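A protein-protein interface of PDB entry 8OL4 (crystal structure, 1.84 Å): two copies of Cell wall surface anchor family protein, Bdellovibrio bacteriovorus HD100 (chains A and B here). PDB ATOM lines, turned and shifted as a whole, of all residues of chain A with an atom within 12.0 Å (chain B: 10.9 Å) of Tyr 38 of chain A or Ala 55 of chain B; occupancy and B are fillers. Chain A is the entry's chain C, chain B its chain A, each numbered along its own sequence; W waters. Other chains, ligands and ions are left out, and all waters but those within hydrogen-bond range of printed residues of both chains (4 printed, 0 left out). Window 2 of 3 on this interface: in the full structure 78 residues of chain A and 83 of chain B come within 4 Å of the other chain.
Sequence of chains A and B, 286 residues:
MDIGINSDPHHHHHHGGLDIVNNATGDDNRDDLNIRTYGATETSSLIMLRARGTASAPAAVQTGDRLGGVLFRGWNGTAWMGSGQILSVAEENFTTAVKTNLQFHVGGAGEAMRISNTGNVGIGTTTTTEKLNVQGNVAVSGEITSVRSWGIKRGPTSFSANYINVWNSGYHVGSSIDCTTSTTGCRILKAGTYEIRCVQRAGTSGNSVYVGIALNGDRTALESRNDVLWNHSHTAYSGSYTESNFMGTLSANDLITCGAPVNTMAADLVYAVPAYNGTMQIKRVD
No position is printed for both chains. Of the 25 pairs that touch across the chains among the printed residues, none has its exchanged pair printed and touching as well.
The side-chain hydroxyl (OG1) of Thr 54 of chain B lies within hydrogen-bond range of the side-chain hydroxyl (OG) of Ser 56 of chain B (2.7 Å). OD2 of Asp 65 of chain B lies within salt-bridge range of NH2 of Arg 50 of chain B (3.999 Å). The guanidinium group (NE) of Arg 52 of chain B lies within salt-bridge range of the side-chain carboxylate (OD2) of Asp 65 of chain B. NH1 of Arg 50 of chain B is in hydrogen-bond range of O of Arg 66 of chain B, at 2.9 Å. The side-chain hydroxyl (OG1) of Thr 54 of chain B lies within hydrogen-bond range of the backbone NH (N) of Ala 57 of chain B (3.0 Å). OG1 of Thr 37 of chain A is in hydrogen-bond range of OG of Ser 44 of chain A (2.6 Å).
Water W4 bridges the guanidinium group of Arg 66 of chain B (2.6 Å) and the side-chain hydroxyl of Ser 45 of chain A (2.9 Å). Water W2 lies within hydrogen-bond range of the backbone carbonyl oxygen of Ala 40 of chain A, the side-chain carboxylate of Asp 65 of chain B and the guanidinium group of Arg 50 of chain B. Water W3 bridges N of Gly 53 of chain B (3.0 Å) and N of Ala 40 of chain A (3.3 Å). Water W1 lies within hydrogen-bond range of the guanidinium group of Arg 52 of chain B (3.1 Å) and the backbone carbonyl oxygen of Ala 40 of chain A (3.1 Å).
Of the 12 printed residues of chain A, 10 touch a printed residue of chain B. Printed residues of chain A that touch a printed residue of chain B: Ile 35, Arg 36, Thr 37, Tyr 38, Gly 39, Ala 40, Thr 41, Glu 42, Thr 43 and Ser 44. Hydrophobic or aromatic side chains of chain A within 4 Å of the printed part of chain B: Ile 35, Tyr 38 and Ala 40. Of the 18 printed residues of chain B, 12 touch a printed residue of chain A. Among the printed residues, no Asp or Glu carboxylate lies within 4 Å of a Lys or Arg side-chain nitrogen of the other chain.
Met 48 of chain B touches Ile 35 of chain A (CA to O, 3.3 Å). CA of Arg 36 of chain A touches O of Leu 49 of chain B, 3.6 Å away. Thr 37 of chain A touches Arg 50 of chain B. O of Ala 51 of chain B touches CA of Tyr 38 of chain A, at 3.2 Å. Gly 53 of chain B touches Tyr 38 of chain A. C of Thr 54 of chain B touches CD2 of Tyr 38 of chain A, at 3.4 Å. Tyr 38 of chain A touches Ala 55 of chain B (CD2 to N, 3.6 Å). Tyr 38 of chain A touches Pro 58 of chain B. N of Gly 39 of chain A touches O of Gly 53 of chain B, 3.5 Å away. Leu 67 of chain B touches Thr 43 of chain A.
The guanidinium group (NH2) of Arg 50 of chain B lies within hydrogen-bond range of the backbone carbonyl oxygen (O) of Ala 40 of chain A, 3.0 Å away. N of Thr 37 of chain A is in hydrogen-bond range of O of Leu 49 of chain B (3.0 Å). The guanidinium group of Arg 52 of chain B sits at hydrogen-bond distance from the backbone carbonyl oxygen of Ala 40 of chain A, at 3.4 Å. The guanidinium group (NE) of Arg 50 of chain B is in hydrogen-bond range of the backbone carbonyl oxygen (O) of Glu 42 of chain A. The backbone carbonyl oxygen of Ser 44 of chain A sits close to the side-chain sulfur of Met 48 of chain B. The guanidinium group (NH2) of Arg 50 of chain B is in hydrogen-bond range of the backbone carbonyl oxygen (O) of Gly 39 of chain A, 2.8 Å away. The backbone carbonyl oxygen (O) of Ala 51 of chain B is in hydrogen-bond range of the backbone NH (N) of Gly 39 of chain A. The backbone NH of Ala 51 of chain B is in hydrogen-bond range of the backbone carbonyl oxygen of Thr 37 of chain A (3.0 Å). The backbone carbonyl oxygen (O) of Ile 35 of chain A is in hydrogen-bond range of the backbone NH (N) of Leu 49 of chain B, 2.8 Å away. OG1 of Thr 43 of chain A lies within hydrogen-bond range of O of Arg 66 of chain B (2.8 Å). The backbone carbonyl oxygen of Leu 49 of chain B is in hydrogen-bond range of the side-chain hydroxyl of Ser 44 of chain A, 3.1 Å away.
Arg 36 of chain A touches just one residue of chain B: Leu 49. Of chain B, only Leu 49, Arg 50 and Ala 51 come within 4 Å of Thr 37 of chain A. Printed residues of chain B within 4 Å of Tyr 38 of chain A: Ala 51, Gly 53, Thr 54, Ala 55 and Pro 58. Gly 39 of chain A touches just these residues of chain B: Arg 50 (2.8 Å), Ala 51 (2.9 Å), Arg 52 (3.7 Å) and Gly 53 (3.5 Å). Of the printed residues of chain B, Ala 40 of chain A touches Arg 50 (3.0 Å) and Arg 52 (3.4 Å). Printed residues of chain A within 4 Å of Arg 52 of chain B: Gly 39 (3.7 Å) and Ala 40 (3.4 Å). Of chain A, only Tyr 38 (3.4 Å) comes within 4 Å of Thr 54 of chain B. Ala 55 of chain B touches just one residue of chain A: Tyr 38 (3.6 Å). No residue of chain A comes within 4 Å of Ser 56 of chain B. No residue of chain A comes within 4 Å of Ala 57 of chain B. The nearest residue of chain A that does not touch Ala 55 of chain B is Arg 36 of chain A (6.2 Å). The nearest printed residue of chain B that does not touch Ser 44 of chain A is Leu 67 of chain B (4.3 Å).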
ATOM      1  N   ASN A  34     -32.660  35.147  15.761  1.00  0.00           N
ATOM      2  CA  ASN A  34     -31.678  34.674  16.723  1.00  0.00           C
ATOM      3  C   ASN A  34     -32.378  34.245  18.000  1.00  0.00           C
ATOM      4  O   ASN A  34     -33.268  34.946  18.492  1.00  0.00           O
ATOM      5  CB  ASN A  34     -30.636  35.749  17.027  1.00  0.00           C
ATOM      6  CG  ASN A  34     -30.105  36.412  15.773  1.00  0.00           C
ATOM      7  OD1 ASN A  34     -30.825  37.144  15.093  1.00  0.00           O
ATOM      8  ND2 ASN A  34     -28.846  36.139  15.445  1.00  0.00           N
ATOM      9  N   ILE A  35     -31.987  33.086  18.516  1.00  0.00           N
ATOM     10  CA  ILE A  35     -32.426  32.595  19.812  1.00  0.00           C
ATOM     11  C   ILE A  35     -31.168  32.408  20.649  1.00  0.00           C
ATOM     12  O   ILE A  35     -30.387  31.480  20.409  1.00  0.00           O
ATOM     13  CB  ILE A  35     -33.213  31.285  19.700  1.00  0.00           C
ATOM     14  CG1 ILE A  35     -34.399  31.443  18.750  1.00  0.00           C
ATOM     15  CG2 ILE A  35     -33.687  30.825  21.076  1.00  0.00           C
ATOM     16  CD1 ILE A  35     -35.196  30.161  18.594  1.00  0.00           C
ATOM     17  N   ARG A  36     -30.976  33.282  21.624  1.00  0.00           N
ATOM     18  CA  ARG A  36     -29.787  33.314  22.462  1.00  0.00           C
ATOM     19  C   ARG A  36     -30.152  32.878  23.876  1.00  0.00           C
ATOM     20  O   ARG A  36     -31.104  33.405  24.464  1.00  0.00           O
ATOM     21  CB  ARG A  36     -29.191  34.723  22.476  1.00  0.00           C
ATOM     22  CG  ARG A  36     -27.933  34.865  23.312  1.00  0.00           C
ATOM     23  CD  ARG A  36     -27.318  36.261  23.175  1.00  0.00           C
ATOM     24  NE  ARG A  36     -27.480  36.796  21.827  1.00  0.00           N
ATOM     25  CZ  ARG A  36     -26.591  37.569  21.208  1.00  0.00           C
ATOM     26  NH1 ARG A  36     -25.451  37.898  21.805  1.00  0.00           N
ATOM     27  NH2 ARG A  36     -26.838  38.005  19.977  1.00  0.00           N
ATOM     28  N   THR A  37     -29.384  31.942  24.429  1.00  0.00           N
ATOM     29  CA  THR A  37     -29.655  31.415  25.764  1.00  0.00           C
ATOM     30  C   THR A  37     -28.373  31.336  26.584  1.00  0.00           C
ATOM     31  O   THR A  37     -27.426  30.645  26.191  1.00  0.00           O
ATOM     32  CB  THR A  37     -30.308  30.036  25.672  1.00  0.00           C
ATOM     33  OG1 THR A  37     -31.480  30.128  24.852  1.00  0.00           O
ATOM     34  CG2 THR A  37     -30.661  29.522  27.061  1.00  0.00           C
ATOM     35  N   TYR A  38     -28.365  32.008  27.736  1.00  0.00           N
ATOM     36  CA  TYR A  38     -27.281  31.927  28.708  1.00  0.00           C
ATOM     37  C   TYR A  38     -27.743  31.101  29.903  1.00  0.00           C
ATOM     38  O   TYR A  38     -28.813  31.364  30.456  1.00  0.00           O
ATOM     39  CB  TYR A  38     -26.861  33.312  29.202  1.00  0.00           C
ATOM     40  CG  TYR A  38     -26.350  34.251  28.146  1.00  0.00           C
ATOM     41  CD1 TYR A  38     -27.226  35.007  27.382  1.00  0.00           C
ATOM     42  CD2 TYR A  38     -24.985  34.401  27.929  1.00  0.00           C
ATOM     43  CE1 TYR A  38     -26.762  35.872  26.410  1.00  0.00           C
ATOM     44  CE2 TYR A  38     -24.508  35.267  26.961  1.00  0.00           C
ATOM     45  CZ  TYR A  38     -25.404  35.995  26.202  1.00  0.00           C
ATOM     46  OH  TYR A  38     -24.928  36.854  25.241  1.00  0.00           O
ATOM     47  N   GLY A  39     -26.945  30.133  30.310  1.00  0.00           N
ATOM     48  CA  GLY A  39     -27.245  29.404  31.528  1.00  0.00           C
ATOM     49  C   GLY A  39     -26.619  28.027  31.520  1.00  0.00           C
ATOM     50  O   GLY A  39     -26.116  27.541  30.507  1.00  0.00           O
ATOM     51  N   ALA A  40     -26.665  27.392  32.697  1.00  0.00           N
ATOM     52  CA  ALA A  40     -26.018  26.100  32.885  1.00  0.00           C
ATOM     53  C   ALA A  40     -26.831  24.952  32.295  1.00  0.00           C
ATOM     54  O   ALA A  40     -26.252  23.965  31.829  1.00  0.00           O
ATOM     55  CB  ALA A  40     -25.767  25.850  34.378  1.00  0.00           C
ATOM     56  N   THR A  41     -28.156  25.050  32.310  1.00  0.00           N
ATOM     57  CA  THR A  41     -28.997  23.981  31.800  1.00  0.00           C
ATOM     58  C   THR A  41     -29.996  24.437  30.750  1.00  0.00           C
ATOM     59  O   THR A  41     -30.629  23.581  30.121  1.00  0.00           O
ATOM     60  CB  THR A  41     -29.760  23.306  32.949  1.00  0.00           C
ATOM     61  OG1 THR A  41     -30.235  24.308  33.857  1.00  0.00           O
ATOM     62  CG2 THR A  41     -28.831  22.345  33.682  1.00  0.00           C
ATOM     63  N   GLU A  42     -30.141  25.737  30.515  1.00  0.00           N
ATOM     64  CA  GLU A  42     -31.099  26.247  29.545  1.00  0.00           C
ATOM     65  C   GLU A  42     -30.516  26.210  28.132  1.00  0.00           C
ATOM     66  O   GLU A  42     -29.313  26.397  27.932  1.00  0.00           O
ATOM     67  CB  GLU A  42     -31.505  27.676  29.910  1.00  0.00           C
ATOM     68  CG  GLU A  42     -32.160  27.819  31.290  1.00  0.00           C
ATOM     69  CD  GLU A  42     -31.160  27.850  32.448  1.00  0.00           C
ATOM     70  OE1 GLU A  42     -29.940  27.684  32.216  1.00  0.00           O
ATOM     71  OE2 GLU A  42     -31.604  28.036  33.601  1.00  0.00           O
ATOM     72  N   THR A  43     -31.385  25.978  27.144  1.00  0.00           N
ATOM     73  CA  THR A  43     -30.951  25.889  25.758  1.00  0.00           C
ATOM     74  C   THR A  43     -31.980  26.593  24.879  1.00  0.00           C
ATOM     75  O   THR A  43     -33.123  26.821  25.291  1.00  0.00           O
ATOM     76  CB  THR A  43     -30.756  24.432  25.315  1.00  0.00           C
ATOM     77  OG1 THR A  43     -30.282  24.417  23.967  1.00  0.00           O
ATOM     78  CG2 THR A  43     -32.092  23.675  25.381  1.00  0.00           C
ATOM     79  N   SER A  44     -31.548  26.970  23.671  1.00  0.00           N
ATOM     80  CA  SER A  44     -32.448  27.592  22.703  1.00  0.00           C
ATOM     81  C   SER A  44     -33.186  26.526  21.904  1.00  0.00           C
ATOM     82  O   SER A  44     -32.591  25.529  21.480  1.00  0.00           O
ATOM     83  CB  SER A  44     -31.678  28.501  21.740  1.00  0.00           C
ATOM     84  OG  SER A  44     -30.847  29.428  22.426  1.00  0.00           O
ATOM     85  N   SER A  45     -34.485  26.749  21.688  1.00  0.00           N
ATOM     86  CA  SER A  45     -35.327  25.803  20.969  1.00  0.00           C
ATOM     87  C   SER A  45     -36.206  26.556  19.978  1.00  0.00           C
ATOM     88  O   SER A  45     -36.794  27.586  20.324  1.00  0.00           O
ATOM     89  CB  SER A  45     -36.220  25.012  21.947  1.00  0.00           C
ATOM     90  OG  SER A  45     -35.452  24.219  22.856  1.00  0.00           O
ATOM     91  N   MET B  48     -29.278  29.753  16.594  1.00  0.00           N
ATOM     92  CA  MET B  48     -29.440  29.422  18.000  1.00  0.00           C
ATOM     93  C   MET B  48     -28.076  29.507  18.672  1.00  0.00           C
ATOM     94  O   MET B  48     -27.127  28.838  18.251  1.00  0.00           O
ATOM     95  CB  MET B  48     -30.061  28.035  18.152  1.00  0.00           C
ATOM     96  CG  MET B  48     -31.572  28.066  18.014  1.00  0.00           C
ATOM     97  SD  MET B  48     -32.327  26.460  17.829  1.00  0.00           S
ATOM     98  CE  MET B  48     -32.134  26.210  16.071  1.00  0.00           C
ATOM     99  N   LEU B  49     -27.983  30.329  19.707  1.00  0.00           N
ATOM    100  CA  LEU B  49     -26.727  30.611  20.388  1.00  0.00           C
ATOM    101  C   LEU B  49     -26.814  30.137  21.833  1.00  0.00           C
ATOM    102  O   LEU B  49     -27.840  30.324  22.500  1.00  0.00           O
ATOM    103  CB  LEU B  49     -26.404  32.106  20.338  1.00  0.00           C
ATOM    104  CG  LEU B  49     -26.331  32.675  18.913  1.00  0.00           C
ATOM    105  CD1 LEU B  49     -27.621  33.424  18.536  1.00  0.00           C
ATOM    106  CD2 LEU B  49     -25.093  33.550  18.726  1.00  0.00           C
ATOM    107  N   ARG B  50     -25.729  29.546  22.323  1.00  0.00           N
ATOM    108  CA  ARG B  50     -25.701  28.990  23.671  1.00  0.00           C
ATOM    109  C   ARG B  50     -24.426  29.424  24.376  1.00  0.00           C
ATOM    110  O   ARG B  50     -23.333  29.326  23.812  1.00  0.00           O
ATOM    111  CB  ARG B  50     -25.798  27.457  23.653  1.00  0.00           C
ATOM    112  CG  ARG B  50     -25.601  26.805  25.039  1.00  0.00           C
ATOM    113  CD  ARG B  50     -26.816  27.033  25.957  1.00  0.00           C
ATOM    114  NE  ARG B  50     -26.572  26.653  27.357  1.00  0.00           N
ATOM    115  CZ  ARG B  50     -26.577  25.399  27.813  1.00  0.00           C
ATOM    116  NH1 ARG B  50     -26.799  24.387  26.984  1.00  0.00           N
ATOM    117  NH2 ARG B  50     -26.368  25.147  29.098  1.00  0.00           N
ATOM    118  N   ALA B  51     -24.571  29.931  25.596  1.00  0.00           N
ATOM    119  CA  ALA B  51     -23.432  30.189  26.463  1.00  0.00           C
ATOM    120  C   ALA B  51     -23.829  29.783  27.873  1.00  0.00           C
ATOM    121  O   ALA B  51     -25.016  29.657  28.184  1.00  0.00           O
ATOM    122  CB  ALA B  51     -22.999  31.666  26.437  1.00  0.00           C
ATOM    123  N   ARG B  52     -22.825  29.565  28.715  1.00  0.00           N
ATOM    124  CA  ARG B  52     -23.033  29.464  30.152  1.00  0.00           C
ATOM    125  C   ARG B  52     -22.929  30.861  30.768  1.00  0.00           C
ATOM    126  O   ARG B  52     -22.694  31.854  30.074  1.00  0.00           O
ATOM    127  CB  ARG B  52     -22.034  28.481  30.765  1.00  0.00           C
ATOM    128  CG  ARG B  52     -22.502  27.046  30.655  1.00  0.00           C
ATOM    129  CD  ARG B  52     -21.497  26.035  31.180  1.00  0.00           C
ATOM    130  NE  ARG B  52     -22.033  24.672  31.050  1.00  0.00           N
ATOM    131  CZ  ARG B  52     -22.581  23.998  32.055  1.00  0.00           C
ATOM    132  NH1 ARG B  52     -22.628  24.549  33.263  1.00  0.00           N
ATOM    133  NH2 ARG B  52     -23.058  22.771  31.858  1.00  0.00           N
ATOM    134  N   GLY B  53     -23.121  30.956  32.083  1.00  0.00           N
ATOM    135  CA  GLY B  53     -23.050  32.265  32.725  1.00  0.00           C
ATOM    136  C   GLY B  53     -24.242  33.134  32.353  1.00  0.00           C
ATOM    137  O   GLY B  53     -25.372  32.655  32.220  1.00  0.00           O
ATOM    138  N   THR B  54     -23.987  34.433  32.170  1.00  0.00           N
ATOM    139  CA  THR B  54     -25.011  35.422  31.860  1.00  0.00           C
ATOM    140  C   THR B  54     -24.544  36.318  30.721  1.00  0.00           C
ATOM    141  O   THR B  54     -23.372  36.324  30.338  1.00  0.00           O
ATOM    142  CB  THR B  54     -25.333  36.308  33.068  1.00  0.00           C
ATOM    143  OG1 THR B  54     -24.146  37.019  33.444  1.00  0.00           O
ATOM    144  CG2 THR B  54     -25.814  35.478  34.229  1.00  0.00           C
ATOM    145  N   ALA B  55     -25.479  37.114  30.194  1.00  0.00           N
ATOM    146  CA  ALA B  55     -25.104  38.099  29.187  1.00  0.00           C
ATOM    147  C   ALA B  55     -24.059  39.064  29.727  1.00  0.00           C
ATOM    148  O   ALA B  55     -23.196  39.527  28.973  1.00  0.00           O
ATOM    149  CB  ALA B  55     -26.340  38.860  28.704  1.00  0.00           C
ATOM    150  N   SER B  56     -24.121  39.377  31.030  1.00  0.00           N
ATOM    151  CA  SER B  56     -23.129  40.239  31.664  1.00  0.00           C
ATOM    152  C   SER B  56     -21.796  39.540  31.893  1.00  0.00           C
ATOM    153  O   SER B  56     -20.764  40.212  31.989  1.00  0.00           O
ATOM    154  CB  SER B  56     -23.659  40.755  33.005  1.00  0.00           C
ATOM    155  OG  SER B  56     -23.976  39.652  33.834  1.00  0.00           O
ATOM    156  N   ALA B  57     -21.782  38.214  31.986  1.00  0.00           N
ATOM    157  CA  ALA B  57     -20.545  37.466  32.219  1.00  0.00           C
ATOM    158  C   ALA B  57     -20.689  36.103  31.569  1.00  0.00           C
ATOM    159  O   ALA B  57     -21.019  35.107  32.227  1.00  0.00           O
ATOM    160  CB  ALA B  57     -20.237  37.342  33.715  1.00  0.00           C
ATOM    161  N   PRO B  58     -20.494  36.031  30.257  1.00  0.00           N
ATOM    162  CA  PRO B  58     -20.682  34.756  29.564  1.00  0.00           C
ATOM    163  C   PRO B  58     -19.554  33.790  29.893  1.00  0.00           C
ATOM    164  O   PRO B  58     -18.426  34.189  30.194  1.00  0.00           O
ATOM    165  CB  PRO B  58     -20.678  35.153  28.085  1.00  0.00           C
ATOM    166  CG  PRO B  58     -19.941  36.454  28.032  1.00  0.00           C
ATOM    167  CD  PRO B  58     -20.260  37.149  29.326  1.00  0.00           C
ATOM    168  N   ALA B  59     -19.883  32.503  29.869  1.00  0.00           N
ATOM    169  CA  ALA B  59     -18.923  31.448  30.145  1.00  0.00           C
ATOM    170  C   ALA B  59     -19.012  30.408  29.042  1.00  0.00           C
ATOM    171  O   ALA B  59     -20.048  30.270  28.382  1.00  0.00           O
ATOM    172  CB  ALA B  59     -19.164  30.794  31.515  1.00  0.00           C
ATOM    173  N   ALA B  60     -17.915  29.672  28.865  1.00  0.00           N
ATOM    174  CA  ALA B  60     -17.784  28.752  27.750  1.00  0.00           C
ATOM    175  C   ALA B  60     -18.737  27.572  27.888  1.00  0.00           C
ATOM    176  O   ALA B  60     -19.043  27.102  28.990  1.00  0.00           O
ATOM    177  CB  ALA B  60     -16.348  28.242  27.639  1.00  0.00           C
ATOM    178  N   VAL B  61     -19.219  27.104  26.738  1.00  0.00           N
ATOM    179  CA  VAL B  61     -20.030  25.904  26.688  1.00  0.00           C
ATOM    180  C   VAL B  61     -19.229  24.700  27.194  1.00  0.00           C
ATOM    181  O   VAL B  61     -18.004  24.631  27.039  1.00  0.00           O
ATOM    182  CB  VAL B  61     -20.499  25.701  25.238  1.00  0.00           C
ATOM    183  CG1 VAL B  61     -21.025  24.291  25.030  1.00  0.00           C
ATOM    184  CG2 VAL B  61     -21.547  26.784  24.862  1.00  0.00           C
ATOM    185  N   ASP B  65     -23.527  20.011  26.875  1.00  0.00           N
ATOM    186  CA  ASP B  65     -24.455  21.130  26.749  1.00  0.00           C
ATOM    187  C   ASP B  65     -25.160  21.109  25.398  1.00  0.00           C
ATOM    188  O   ASP B  65     -24.512  20.978  24.355  1.00  0.00           O
ATOM    189  CB  ASP B  65     -23.712  22.451  26.879  1.00  0.00           C
ATOM    190  CG  ASP B  65     -23.354  22.780  28.295  1.00  0.00           C
ATOM    191  OD1 ASP B  65     -23.784  22.043  29.209  1.00  0.00           O
ATOM    192  OD2 ASP B  65     -22.655  23.795  28.483  1.00  0.00           O
ATOM    193  N   ARG B  66     -26.484  21.287  25.389  1.00  0.00           N
ATOM    194  CA  ARG B  66     -27.234  21.393  24.113  1.00  0.00           C
ATOM    195  C   ARG B  66     -27.077  22.812  23.570  1.00  0.00           C
ATOM    196  O   ARG B  66     -27.531  23.728  24.211  1.00  0.00           O
ATOM    197  CB  ARG B  66     -28.730  21.100  24.237  1.00  0.00           C
ATOM    198  CG  ARG B  66     -29.399  20.877  22.887  1.00  0.00           C
ATOM    199  CD  ARG B  66     -30.894  20.668  22.972  1.00  0.00           C
ATOM    200  NE  ARG B  66     -31.270  19.467  23.694  1.00  0.00           N
ATOM    201  CZ  ARG B  66     -32.520  19.094  23.943  1.00  0.00           C
ATOM    202  NH1 ARG B  66     -33.525  19.770  23.422  1.00  0.00           N
ATOM    203  NH2 ARG B  66     -32.785  18.008  24.640  1.00  0.00           N
ATOM    204  N   LEU B  67     -26.484  22.971  22.400  1.00  0.00           N
ATOM    205  CA  LEU B  67     -26.391  24.276  21.749  1.00  0.00           C
ATOM    206  C   LEU B  67     -27.767  24.789  21.343  1.00  0.00           C
ATOM    207  O   LEU B  67     -28.054  25.985  21.455  1.00  0.00           O
ATOM    208  CB  LEU B  67     -25.497  24.180  20.515  1.00  0.00           C
ATOM    209  CG  LEU B  67     -23.987  24.067  20.712  1.00  0.00           C
ATOM    210  CD1 LEU B  67     -23.507  25.163  21.682  1.00  0.00           C
ATOM    211  CD2 LEU B  67     -23.595  22.660  21.176  1.00  0.00           C
ATOM    212  N   GLY B  68     -28.611  23.907  20.834  1.00  0.00           N
ATOM    213  CA  GLY B  68     -29.941  24.297  20.408  1.00  0.00           C
ATOM    214  C   GLY B  68     -30.621  23.085  19.816  1.00  0.00           C
ATOM    215  O   GLY B  68     -30.019  22.013  19.683  1.00  0.00           O
HETATM  216  O   HOH W   1     -25.302  21.583  33.653  1.00  0.00           O
HETATM  217  O   HOH W   2     -26.552  21.885  30.304  1.00  0.00           O
HETATM  218  O   HOH W   3     -23.919  28.766  33.949  1.00  0.00           O
HETATM  219  O   HOH W   4     -33.408  22.198  22.521  1.00  0.00           O
